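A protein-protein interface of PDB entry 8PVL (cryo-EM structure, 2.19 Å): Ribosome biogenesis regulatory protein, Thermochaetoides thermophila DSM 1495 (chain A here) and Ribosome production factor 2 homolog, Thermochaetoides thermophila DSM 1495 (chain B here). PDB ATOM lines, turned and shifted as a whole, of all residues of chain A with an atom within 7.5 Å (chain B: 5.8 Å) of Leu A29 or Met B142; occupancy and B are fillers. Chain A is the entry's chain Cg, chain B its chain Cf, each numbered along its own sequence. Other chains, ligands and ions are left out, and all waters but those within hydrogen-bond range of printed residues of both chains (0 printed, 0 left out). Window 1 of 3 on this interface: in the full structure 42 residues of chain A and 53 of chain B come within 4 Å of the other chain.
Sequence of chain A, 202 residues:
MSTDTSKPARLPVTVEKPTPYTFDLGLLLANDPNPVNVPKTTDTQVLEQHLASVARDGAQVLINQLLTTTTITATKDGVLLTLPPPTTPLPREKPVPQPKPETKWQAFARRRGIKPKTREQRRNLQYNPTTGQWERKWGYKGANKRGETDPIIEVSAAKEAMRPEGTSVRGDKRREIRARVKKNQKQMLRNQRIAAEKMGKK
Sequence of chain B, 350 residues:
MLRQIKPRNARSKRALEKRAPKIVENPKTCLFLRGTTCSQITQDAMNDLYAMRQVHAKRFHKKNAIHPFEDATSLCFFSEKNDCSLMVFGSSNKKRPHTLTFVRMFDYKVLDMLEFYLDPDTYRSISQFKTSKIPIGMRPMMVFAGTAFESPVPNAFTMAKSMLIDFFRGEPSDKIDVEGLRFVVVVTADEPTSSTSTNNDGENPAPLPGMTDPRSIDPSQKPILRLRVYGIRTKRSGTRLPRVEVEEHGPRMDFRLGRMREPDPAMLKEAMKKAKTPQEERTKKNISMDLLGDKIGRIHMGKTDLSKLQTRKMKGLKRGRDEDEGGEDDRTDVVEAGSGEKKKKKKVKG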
ATOM      1  N   THR A  22     -12.000  -8.416   3.112  1.00  0.00           N
ATOM      2  CA  THR A  22     -12.016  -9.740   3.714  1.00  0.00           C
ATOM      3  C   THR A  22     -13.461 -10.182   3.898  1.00  0.00           C
ATOM      4  O   THR A  22     -14.380  -9.362   3.917  1.00  0.00           O
ATOM      5  CB  THR A  22     -11.264  -9.762   5.049  1.00  0.00           C
ATOM      6  OG1 THR A  22     -11.294  -8.459   5.642  1.00  0.00           O
ATOM      7  CG2 THR A  22      -9.820 -10.184   4.840  1.00  0.00           C
ATOM      8  N   PHE A  23     -13.669 -11.489   4.015  1.00  0.00           N
ATOM      9  CA  PHE A  23     -15.024 -12.018   3.997  1.00  0.00           C
ATOM     10  C   PHE A  23     -15.215 -13.075   5.071  1.00  0.00           C
ATOM     11  O   PHE A  23     -14.275 -13.769   5.467  1.00  0.00           O
ATOM     12  CB  PHE A  23     -15.373 -12.618   2.631  1.00  0.00           C
ATOM     13  CG  PHE A  23     -15.509 -11.599   1.543  1.00  0.00           C
ATOM     14  CD1 PHE A  23     -16.701 -10.920   1.358  1.00  0.00           C
ATOM     15  CD2 PHE A  23     -14.446 -11.319   0.701  1.00  0.00           C
ATOM     16  CE1 PHE A  23     -16.829  -9.979   0.357  1.00  0.00           C
ATOM     17  CE2 PHE A  23     -14.569 -10.380  -0.302  1.00  0.00           C
ATOM     18  CZ  PHE A  23     -15.762  -9.710  -0.475  1.00  0.00           C
ATOM     19  N   ASP A  24     -16.460 -13.178   5.539  1.00  0.00           N
ATOM     20  CA  ASP A  24     -16.933 -14.291   6.364  1.00  0.00           C
ATOM     21  C   ASP A  24     -18.330 -14.609   5.834  1.00  0.00           C
ATOM     22  O   ASP A  24     -19.320 -13.999   6.246  1.00  0.00           O
ATOM     23  CB  ASP A  24     -16.938 -13.944   7.845  1.00  0.00           C
ATOM     24  CG  ASP A  24     -17.263 -15.135   8.719  1.00  0.00           C
ATOM     25  OD1 ASP A  24     -18.103 -14.994   9.627  1.00  0.00           O
ATOM     26  OD2 ASP A  24     -16.677 -16.214   8.497  1.00  0.00           O
ATOM     27  N   LEU A  25     -18.396 -15.541   4.885  1.00  0.00           N
ATOM     28  CA  LEU A  25     -19.641 -15.831   4.189  1.00  0.00           C
ATOM     29  C   LEU A  25     -20.628 -16.622   5.035  1.00  0.00           C
ATOM     30  O   LEU A  25     -21.805 -16.700   4.666  1.00  0.00           O
ATOM     31  CB  LEU A  25     -19.351 -16.584   2.888  1.00  0.00           C
ATOM     32  CG  LEU A  25     -18.538 -15.814   1.844  1.00  0.00           C
ATOM     33  CD1 LEU A  25     -18.502 -16.567   0.526  1.00  0.00           C
ATOM     34  CD2 LEU A  25     -19.094 -14.412   1.644  1.00  0.00           C
ATOM     35  N   GLY A  26     -20.184 -17.214   6.144  1.00  0.00           N
ATOM     36  CA  GLY A  26     -21.118 -17.819   7.075  1.00  0.00           C
ATOM     37  C   GLY A  26     -22.023 -16.803   7.741  1.00  0.00           C
ATOM     38  O   GLY A  26     -23.192 -17.092   8.012  1.00  0.00           O
ATOM     39  N   LEU A  27     -21.502 -15.609   8.014  1.00  0.00           N
ATOM     40  CA  LEU A  27     -22.275 -14.528   8.606  1.00  0.00           C
ATOM     41  C   LEU A  27     -22.691 -13.477   7.587  1.00  0.00           C
ATOM     42  O   LEU A  27     -23.275 -12.459   7.977  1.00  0.00           O
ATOM     43  CB  LEU A  27     -21.480 -13.870   9.735  1.00  0.00           C
ATOM     44  CG  LEU A  27     -21.124 -14.771  10.916  1.00  0.00           C
ATOM     45  CD1 LEU A  27     -20.341 -14.001  11.963  1.00  0.00           C
ATOM     46  CD2 LEU A  27     -22.373 -15.379  11.515  1.00  0.00           C
ATOM     47  N   LEU A  28     -22.413 -13.712   6.300  1.00  0.00           N
ATOM     48  CA  LEU A  28     -22.649 -12.758   5.210  1.00  0.00           C
ATOM     49  C   LEU A  28     -21.986 -11.412   5.500  1.00  0.00           C
ATOM     50  O   LEU A  28     -22.575 -10.346   5.313  1.00  0.00           O
ATOM     51  CB  LEU A  28     -24.144 -12.583   4.934  1.00  0.00           C
ATOM     52  CG  LEU A  28     -25.018 -13.835   4.886  1.00  0.00           C
ATOM     53  CD1 LEU A  28     -26.480 -13.446   4.991  1.00  0.00           C
ATOM     54  CD2 LEU A  28     -24.762 -14.624   3.614  1.00  0.00           C
ATOM     55  N   LEU A  29     -20.743 -11.470   5.968  1.00  0.00           N
ATOM     56  CA  LEU A  29     -20.024 -10.301   6.450  1.00  0.00           C
ATOM     57  C   LEU A  29     -18.885  -9.960   5.502  1.00  0.00           C
ATOM     58  O   LEU A  29     -18.119 -10.842   5.100  1.00  0.00           O
ATOM     59  CB  LEU A  29     -19.482 -10.556   7.858  1.00  0.00           C
ATOM     60  CG  LEU A  29     -18.429  -9.592   8.395  1.00  0.00           C
ATOM     61  CD1 LEU A  29     -19.034  -8.221   8.594  1.00  0.00           C
ATOM     62  CD2 LEU A  29     -17.841 -10.113   9.691  1.00  0.00           C
ATOM     63  N   ALA A  30     -18.777  -8.681   5.148  1.00  0.00           N
ATOM     64  CA  ALA A  30     -17.653  -8.161   4.381  1.00  0.00           C
ATOM     65  C   ALA A  30     -16.943  -7.097   5.204  1.00  0.00           C
ATOM     66  O   ALA A  30     -17.575  -6.150   5.680  1.00  0.00           O
ATOM     67  CB  ALA A  30     -18.111  -7.574   3.045  1.00  0.00           C
ATOM     68  N   ASN A  31     -15.635  -7.255   5.368  1.00  0.00           N
ATOM     69  CA  ASN A  31     -14.809  -6.312   6.104  1.00  0.00           C
ATOM     70  C   ASN A  31     -14.025  -5.474   5.105  1.00  0.00           C
ATOM     71  O   ASN A  31     -13.305  -6.020   4.258  1.00  0.00           O
ATOM     72  CB  ASN A  31     -13.861  -7.045   7.051  1.00  0.00           C
ATOM     73  CG  ASN A  31     -14.514  -7.404   8.365  1.00  0.00           C
ATOM     74  OD1 ASN A  31     -15.317  -6.642   8.901  1.00  0.00           O
ATOM     75  ND2 ASN A  31     -14.177  -8.574   8.892  1.00  0.00           N
ATOM     76  N   ASP A  32     -14.166  -4.150   5.209  1.00  0.00           N
ATOM     77  CA  ASP A  32     -13.493  -3.219   4.318  1.00  0.00           C
ATOM     78  C   ASP A  32     -12.347  -2.560   5.066  1.00  0.00           C
ATOM     79  O   ASP A  32     -12.595  -1.697   5.923  1.00  0.00           O
ATOM     80  CB  ASP A  32     -14.471  -2.165   3.806  1.00  0.00           C
ATOM     81  CG  ASP A  32     -13.830  -1.198   2.830  1.00  0.00           C
ATOM     82  OD1 ASP A  32     -12.876  -1.598   2.133  1.00  0.00           O
ATOM     83  OD2 ASP A  32     -14.284  -0.037   2.756  1.00  0.00           O
ATOM     84  N   GLY A  58     -19.446  -2.161  -0.983  1.00  0.00           N
ATOM     85  CA  GLY A  58     -19.488  -3.308  -0.085  1.00  0.00           C
ATOM     86  C   GLY A  58     -20.507  -4.354  -0.502  1.00  0.00           C
ATOM     87  O   GLY A  58     -20.209  -5.555  -0.527  1.00  0.00           O
ATOM     88  N   ALA A  59     -21.715  -3.912  -0.860  1.00  0.00           N
ATOM     89  CA  ALA A  59     -22.747  -4.837  -1.316  1.00  0.00           C
ATOM     90  C   ALA A  59     -22.353  -5.506  -2.624  1.00  0.00           C
ATOM     91  O   ALA A  59     -22.611  -6.700  -2.818  1.00  0.00           O
ATOM     92  CB  ALA A  59     -24.080  -4.106  -1.467  1.00  0.00           C
ATOM     93  N   LEU A  62     -19.701  -8.158  -1.903  1.00  0.00           N
ATOM     94  CA  LEU A  62     -20.329  -9.285  -1.217  1.00  0.00           C
ATOM     95  C   LEU A  62     -21.134 -10.148  -2.182  1.00  0.00           C
ATOM     96  O   LEU A  62     -21.069 -11.383  -2.121  1.00  0.00           O
ATOM     97  CB  LEU A  62     -21.219  -8.779  -0.083  1.00  0.00           C
ATOM     98  CG  LEU A  62     -20.892  -9.304   1.314  1.00  0.00           C
ATOM     99  CD1 LEU A  62     -21.906  -8.809   2.322  1.00  0.00           C
ATOM    100  CD2 LEU A  62     -20.832 -10.821   1.320  1.00  0.00           C
ATOM    101  N   GLN A  65     -18.670 -12.126  -4.399  1.00  0.00           N
ATOM    102  CA  GLN A  65     -18.066 -13.241  -3.675  1.00  0.00           C
ATOM    103  C   GLN A  65     -19.060 -14.377  -3.465  1.00  0.00           C
ATOM    104  O   GLN A  65     -18.715 -15.552  -3.644  1.00  0.00           O
ATOM    105  CB  GLN A  65     -17.517 -12.756  -2.334  1.00  0.00           C
ATOM    106  CG  GLN A  65     -16.670 -13.780  -1.602  1.00  0.00           C
ATOM    107  CD  GLN A  65     -15.238 -13.813  -2.093  1.00  0.00           C
ATOM    108  OE1 GLN A  65     -14.831 -12.994  -2.916  1.00  0.00           O
ATOM    109  NE2 GLN A  65     -14.462 -14.763  -1.588  1.00  0.00           N
ATOM    110  N   LEU A  66     -20.305 -14.045  -3.103  1.00  0.00           N
ATOM    111  CA  LEU A  66     -21.309 -15.079  -2.871  1.00  0.00           C
ATOM    112  C   LEU A  66     -21.684 -15.797  -4.160  1.00  0.00           C
ATOM    113  O   LEU A  66     -21.933 -17.009  -4.152  1.00  0.00           O
ATOM    114  CB  LEU A  66     -22.549 -14.471  -2.219  1.00  0.00           C
ATOM    115  CG  LEU A  66     -22.441 -14.180  -0.722  1.00  0.00           C
ATOM    116  CD1 LEU A  66     -23.491 -13.171  -0.295  1.00  0.00           C
ATOM    117  CD2 LEU A  66     -22.571 -15.461   0.078  1.00  0.00           C
ATOM    118  N   THR A  88     -15.691 -15.918  11.968  1.00  0.00           N
ATOM    119  CA  THR A  88     -15.493 -14.785  12.862  1.00  0.00           C
ATOM    120  C   THR A  88     -15.678 -15.242  14.303  1.00  0.00           C
ATOM    121  O   THR A  88     -16.729 -15.806  14.633  1.00  0.00           O
ATOM    122  CB  THR A  88     -16.469 -13.661  12.529  1.00  0.00           C
ATOM    123  OG1 THR A  88     -16.224 -13.194  11.198  1.00  0.00           O
ATOM    124  CG2 THR A  88     -16.299 -12.503  13.501  1.00  0.00           C
ATOM    125  N   PRO B 140     -29.996  -9.754   7.292  1.00  0.00           N
ATOM    126  CA  PRO B 140     -29.349  -9.003   6.216  1.00  0.00           C
ATOM    127  C   PRO B 140     -27.870  -9.355   6.083  1.00  0.00           C
ATOM    128  O   PRO B 140     -27.270  -9.986   6.954  1.00  0.00           O
ATOM    129  CB  PRO B 140     -29.523  -7.551   6.672  1.00  0.00           C
ATOM    130  CG  PRO B 140     -29.466  -7.640   8.165  1.00  0.00           C
ATOM    131  CD  PRO B 140     -30.022  -8.993   8.554  1.00  0.00           C
ATOM    132  N   MET B 141     -27.294  -8.930   4.963  1.00  0.00           N
ATOM    133  CA  MET B 141     -25.850  -8.980   4.812  1.00  0.00           C
ATOM    134  C   MET B 141     -25.216  -7.823   5.578  1.00  0.00           C
ATOM    135  O   MET B 141     -25.891  -6.894   6.022  1.00  0.00           O
ATOM    136  CB  MET B 141     -25.455  -8.935   3.338  1.00  0.00           C
ATOM    137  CG  MET B 141     -26.212  -9.914   2.461  1.00  0.00           C
ATOM    138  SD  MET B 141     -26.632  -9.236   0.846  1.00  0.00           S
ATOM    139  CE  MET B 141     -25.154  -8.300   0.471  1.00  0.00           C
ATOM    140  N   MET B 142     -23.899  -7.884   5.746  1.00  0.00           N
ATOM    141  CA  MET B 142     -23.206  -6.943   6.610  1.00  0.00           C
ATOM    142  C   MET B 142     -21.931  -6.430   5.963  1.00  0.00           C
ATOM    143  O   MET B 142     -21.196  -7.187   5.324  1.00  0.00           O
ATOM    144  CB  MET B 142     -22.867  -7.586   7.938  1.00  0.00           C
ATOM    145  CG  MET B 142     -24.013  -7.592   8.897  1.00  0.00           C
ATOM    146  SD  MET B 142     -23.849  -8.953  10.042  1.00  0.00           S
ATOM    147  CE  MET B 142     -23.587  -7.989  11.505  1.00  0.00           C
ATOM    148  N   VAL B 143     -21.673  -5.137   6.148  1.00  0.00           N
ATOM    149  CA  VAL B 143     -20.451  -4.487   5.691  1.00  0.00           C
ATOM    150  C   VAL B 143     -19.924  -3.635   6.837  1.00  0.00           C
ATOM    151  O   VAL B 143     -20.655  -2.798   7.379  1.00  0.00           O
ATOM    152  CB  VAL B 143     -20.687  -3.626   4.439  1.00  0.00           C
ATOM    153  CG1 VAL B 143     -19.474  -2.764   4.148  1.00  0.00           C
ATOM    154  CG2 VAL B 143     -21.013  -4.499   3.236  1.00  0.00           C
ATOM    155  N   PHE B 144     -18.670  -3.861   7.219  1.00  0.00           N
ATOM    156  CA  PHE B 144     -17.968  -3.018   8.178  1.00  0.00           C
ATOM    157  C   PHE B 144     -16.840  -2.306   7.444  1.00  0.00           C
ATOM    158  O   PHE B 144     -15.995  -2.956   6.821  1.00  0.00           O
ATOM    159  CB  PHE B 144     -17.430  -3.838   9.349  1.00  0.00           C
ATOM    160  CG  PHE B 144     -18.447  -4.100  10.423  1.00  0.00           C
ATOM    161  CD1 PHE B 144     -19.384  -5.109  10.276  1.00  0.00           C
ATOM    162  CD2 PHE B 144     -18.472  -3.334  11.575  1.00  0.00           C
ATOM    163  CE1 PHE B 144     -20.321  -5.354  11.258  1.00  0.00           C
ATOM    164  CE2 PHE B 144     -19.409  -3.573  12.563  1.00  0.00           C
ATOM    165  CZ  PHE B 144     -20.334  -4.586  12.404  1.00  0.00           C
ATOM    166  N   LYS B 161     -17.837  -3.626  17.003  1.00  0.00           N
ATOM    167  CA  LYS B 161     -17.999  -4.508  15.852  1.00  0.00           C
ATOM    168  C   LYS B 161     -18.470  -5.892  16.279  1.00  0.00           C
ATOM    169  O   LYS B 161     -19.379  -6.462  15.661  1.00  0.00           O
ATOM    170  CB  LYS B 161     -16.687  -4.608  15.074  1.00  0.00           C
ATOM    171  CG  LYS B 161     -16.736  -5.590  13.917  1.00  0.00           C
ATOM    172  CD  LYS B 161     -15.381  -5.760  13.267  1.00  0.00           C
ATOM    173  CE  LYS B 161     -15.420  -6.843  12.205  1.00  0.00           C
ATOM    174  NZ  LYS B 161     -14.089  -7.051  11.579  1.00  0.00           N
ATOM    175  N   LEU B 164     -22.189  -5.601  17.384  1.00  0.00           N
ATOM    176  CA  LEU B 164     -23.109  -5.433  16.266  1.00  0.00           C
ATOM    177  C   LEU B 164     -23.201  -6.697  15.421  1.00  0.00           C
ATOM    178  O   LEU B 164     -24.264  -6.982  14.854  1.00  0.00           O
ATOM    179  CB  LEU B 164     -22.691  -4.233  15.419  1.00  0.00           C
ATOM    180  CG  LEU B 164     -22.908  -2.884  16.110  1.00  0.00           C
ATOM    181  CD1 LEU B 164     -22.268  -1.751  15.326  1.00  0.00           C
ATOM    182  CD2 LEU B 164     -24.387  -2.619  16.330  1.00  0.00           C
ATOM    183  N   ILE B 165     -22.116  -7.474  15.342  1.00  0.00           N
ATOM    184  CA  ILE B 165     -22.193  -8.776  14.686  1.00  0.00           C
ATOM    185  C   ILE B 165     -23.110  -9.713  15.464  1.00  0.00           C
ATOM    186  O   ILE B 165     -23.971 -10.384  14.879  1.00  0.00           O
ATOM    187  CB  ILE B 165     -20.786  -9.367  14.486  1.00  0.00           C
ATOM    188  CG1 ILE B 165     -20.066  -8.635  13.354  1.00  0.00           C
ATOM    189  CG2 ILE B 165     -20.856 -10.841  14.145  1.00  0.00           C
ATOM    190  CD1 ILE B 165     -18.612  -9.011  13.218  1.00  0.00           C
ATOM    191  N   ASP B 166     -22.974  -9.740  16.793  1.00  0.00           N
ATOM    192  CA  ASP B 166     -23.862 -10.568  17.606  1.00  0.00           C
ATOM    193  C   ASP B 166     -25.309 -10.084  17.547  1.00  0.00           C
ATOM    194  O   ASP B 166     -26.236 -10.882  17.722  1.00  0.00           O
ATOM    195  CB  ASP B 166     -23.375 -10.602  19.052  1.00  0.00           C
ATOM    196  CG  ASP B 166     -23.298 -12.009  19.603  1.00  0.00           C
ATOM    197  OD1 ASP B 166     -23.977 -12.899  19.054  1.00  0.00           O
ATOM    198  OD2 ASP B 166     -22.556 -12.231  20.580  1.00  0.00           O
ATOM    199  N   PHE B 168     -26.894  -8.292  14.746  1.00  0.00           N
ATOM    200  CA  PHE B 168     -27.465  -8.536  13.428  1.00  0.00           C
ATOM    201  C   PHE B 168     -27.093  -9.905  12.865  1.00  0.00           C
ATOM    202  O   PHE B 168     -27.231 -10.120  11.657  1.00  0.00           O
ATOM    203  CB  PHE B 168     -27.025  -7.447  12.448  1.00  0.00           C
ATOM    204  CG  PHE B 168     -27.533  -6.076  12.785  1.00  0.00           C
ATOM    205  CD1 PHE B 168     -28.818  -5.691  12.443  1.00  0.00           C
ATOM    206  CD2 PHE B 168     -26.715  -5.165  13.433  1.00  0.00           C
ATOM    207  CE1 PHE B 168     -29.279  -4.425  12.750  1.00  0.00           C
ATOM    208  CE2 PHE B 168     -27.169  -3.902  13.742  1.00  0.00           C
ATOM    209  CZ  PHE B 168     -28.453  -3.532  13.400  1.00  0.00           C
ATOM    210  N   ARG B 169     -26.611 -10.819  13.712  1.00  0.00           N
ATOM    211  CA  ARG B 169     -26.177 -12.136  13.251  1.00  0.00           C
ATOM    212  C   ARG B 169     -27.334 -12.950  12.682  1.00  0.00           C
ATOM    213  O   ARG B 169     -27.227 -13.521  11.591  1.00  0.00           O
ATOM    214  CB  ARG B 169     -25.513 -12.881  14.409  1.00  0.00           C
ATOM    215  CG  ARG B 169     -24.852 -14.188  14.036  1.00  0.00           C
ATOM    216  CD  ARG B 169     -24.316 -14.886  15.288  1.00  0.00           C
ATOM    217  NE  ARG B 169     -23.380 -15.980  15.035  1.00  0.00           N
ATOM    218  CZ  ARG B 169     -23.643 -17.097  14.367  1.00  0.00           C
ATOM    219  NH1 ARG B 169     -24.862 -17.387  13.939  1.00  0.00           N
ATOM    220  NH2 ARG B 169     -22.661 -17.967  14.152  1.00  0.00           N
ATOM    221  N   PHE B 183     -30.997  -6.967   1.523  1.00  0.00           N
ATOM    222  CA  PHE B 183     -30.766  -5.891   2.475  1.00  0.00           C
ATOM    223  C   PHE B 183     -29.375  -6.018   3.076  1.00  0.00           C
ATOM    224  O   PHE B 183     -28.916  -7.125   3.372  1.00  0.00           O
ATOM    225  CB  PHE B 183     -31.833  -5.894   3.578  1.00  0.00           C
ATOM    226  CG  PHE B 183     -33.210  -5.566   3.078  1.00  0.00           C
ATOM    227  CD1 PHE B 183     -33.622  -4.250   2.960  1.00  0.00           C
ATOM    228  CD2 PHE B 183     -34.084  -6.574   2.703  1.00  0.00           C
ATOM    229  CE1 PHE B 183     -34.884  -3.944   2.490  1.00  0.00           C
ATOM    230  CE2 PHE B 183     -35.344  -6.276   2.227  1.00  0.00           C
ATOM    231  CZ  PHE B 183     -35.745  -4.959   2.120  1.00  0.00           C
ATOM    232  N   VAL B 184     -28.713  -4.878   3.263  1.00  0.00           N
ATOM    233  CA  VAL B 184     -27.355  -4.830   3.790  1.00  0.00           C
ATOM    234  C   VAL B 184     -27.292  -3.785   4.899  1.00  0.00           C
ATOM    235  O   VAL B 184     -27.955  -2.744   4.834  1.00  0.00           O
ATOM    236  CB  VAL B 184     -26.323  -4.550   2.667  1.00  0.00           C
ATOM    237  CG1 VAL B 184     -26.565  -3.202   1.994  1.00  0.00           C
ATOM    238  CG2 VAL B 184     -24.889  -4.675   3.175  1.00  0.00           C
ATOM    239  N   VAL B 185     -26.537  -4.096   5.949  1.00  0.00           N
ATOM    240  CA  VAL B 185     -26.318  -3.208   7.085  1.00  0.00           C
ATOM    241  C   VAL B 185     -24.854  -2.795   7.068  1.00  0.00           C
ATOM    242  O   VAL B 185     -23.961  -3.651   7.109  1.00  0.00           O
ATOM    243  CB  VAL B 185     -26.685  -3.895   8.410  1.00  0.00           C
ATOM    244  CG1 VAL B 185     -26.178  -3.091   9.585  1.00  0.00           C
ATOM    245  CG2 VAL B 185     -28.187  -4.090   8.505  1.00  0.00           C
ATOM    246  N   VAL B 186     -24.601  -1.490   7.009  1.00  0.00           N
ATOM    247  CA  VAL B 186     -23.258  -0.950   6.843  1.00  0.00           C
ATOM    248  C   VAL B 186     -22.908  -0.119   8.069  1.00  0.00           C
ATOM    249  O   VAL B 186     -23.641   0.810   8.433  1.00  0.00           O
ATOM    250  CB  VAL B 186     -23.137  -0.115   5.560  1.00  0.00           C
ATOM    251  CG1 VAL B 186     -21.738   0.458   5.428  1.00  0.00           C
ATOM    252  CG2 VAL B 186     -23.473  -0.972   4.355  1.00  0.00           C
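The backbone NH (N) of Asp A32 is in hydrogen-bond range of the backbone carbonyl oxygen (O) of Phe B144 (2.7 Å).
O of Leu A28 lies within hydrogen-bond range of N of Met B142 (2.8 Å).
N of Ala A30 lies within hydrogen-bond range of O of Met B142, at 2.8 Å.
The side-chain amino group (NZ) of Lys B161 lies within hydrogen-bond range of the side-chain amide oxygen (OD1) of Asn A31, 3.0 Å away.
The backbone carbonyl oxygen of Ala A30 sits at hydrogen-bond distance from the backbone NH of Phe B144 (3.0 Å).
The backbone NH of Met B141 is in hydrogen-bond range of the backbone carbonyl oxygen of Phe B183.
The backbone NH (N) of Val B143 lies within hydrogen-bond range of the backbone carbonyl oxygen (O) of Val B185 (2.9 Å).
The backbone carbonyl oxygen (O) of Thr A22 is in hydrogen-bond range of the backbone NH (N) of Asn A31.
The backbone carbonyl oxygen (O) of Leu A29 sits at hydrogen-bond distance from the backbone NH (N) of Asp A24.
The backbone carbonyl oxygen of Met B141 sits at hydrogen-bond distance from the backbone NH of Val B185, at 2.9 Å.
Leu A27 touches Ile B165.
CD2 of Leu A27 touches CZ of Arg B169 (3.6 Å).
O of Leu A28 touches CA of Met B141, 3.6 Å away.
Phe B144 touches Leu A29 (CD1 to CD1, 3.6 Å).
CD2 of Leu A29 touches CD1 of Ile B165, 3.8 Å away.
Ala A30 touches Val B143.
CB of Phe B144 touches OD1 of Asn A31, at 3.5 Å.
Gly A58 touches Val B143 (C to CG2, 3.8 Å).
Leu A62 touches Met B141.
Met B142 touches Leu A62 (O to CD1, 3.5 Å).
Of chain B, only Met B142 (3.5 Å), Phe B144 (3.6 Å) and Ile B165 (3.8 Å) come within 4 Å of Leu A29.
Met B142 touches four residues of chain A.
Of the printed residues of chain A, Arg B169 touches Leu A27.
Printed residues of chain B within 4 Å of Leu A27: Ile B165 and Arg B169.
Printed residues of chain A within 4 Å of Ile B165: Leu A27 and Leu A29.
Of the printed residues of chain B, Leu A62 touches Met B141 (3.7 Å) and Met B142 (3.5 Å).
The nearest residue of chain B that does not touch Leu A29 is Val B143 (4.7 Å).
The nearest residue of chain A that does not touch Met B142 is Leu A27 (4.1 Å).
Of the 15 printed residues of chain B, 7 touch a printed residue of chain A.
Among the printed residues, no Asp or Glu carboxylate lies within 4 Å of a Lys or Arg side-chain nitrogen of the other chain.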
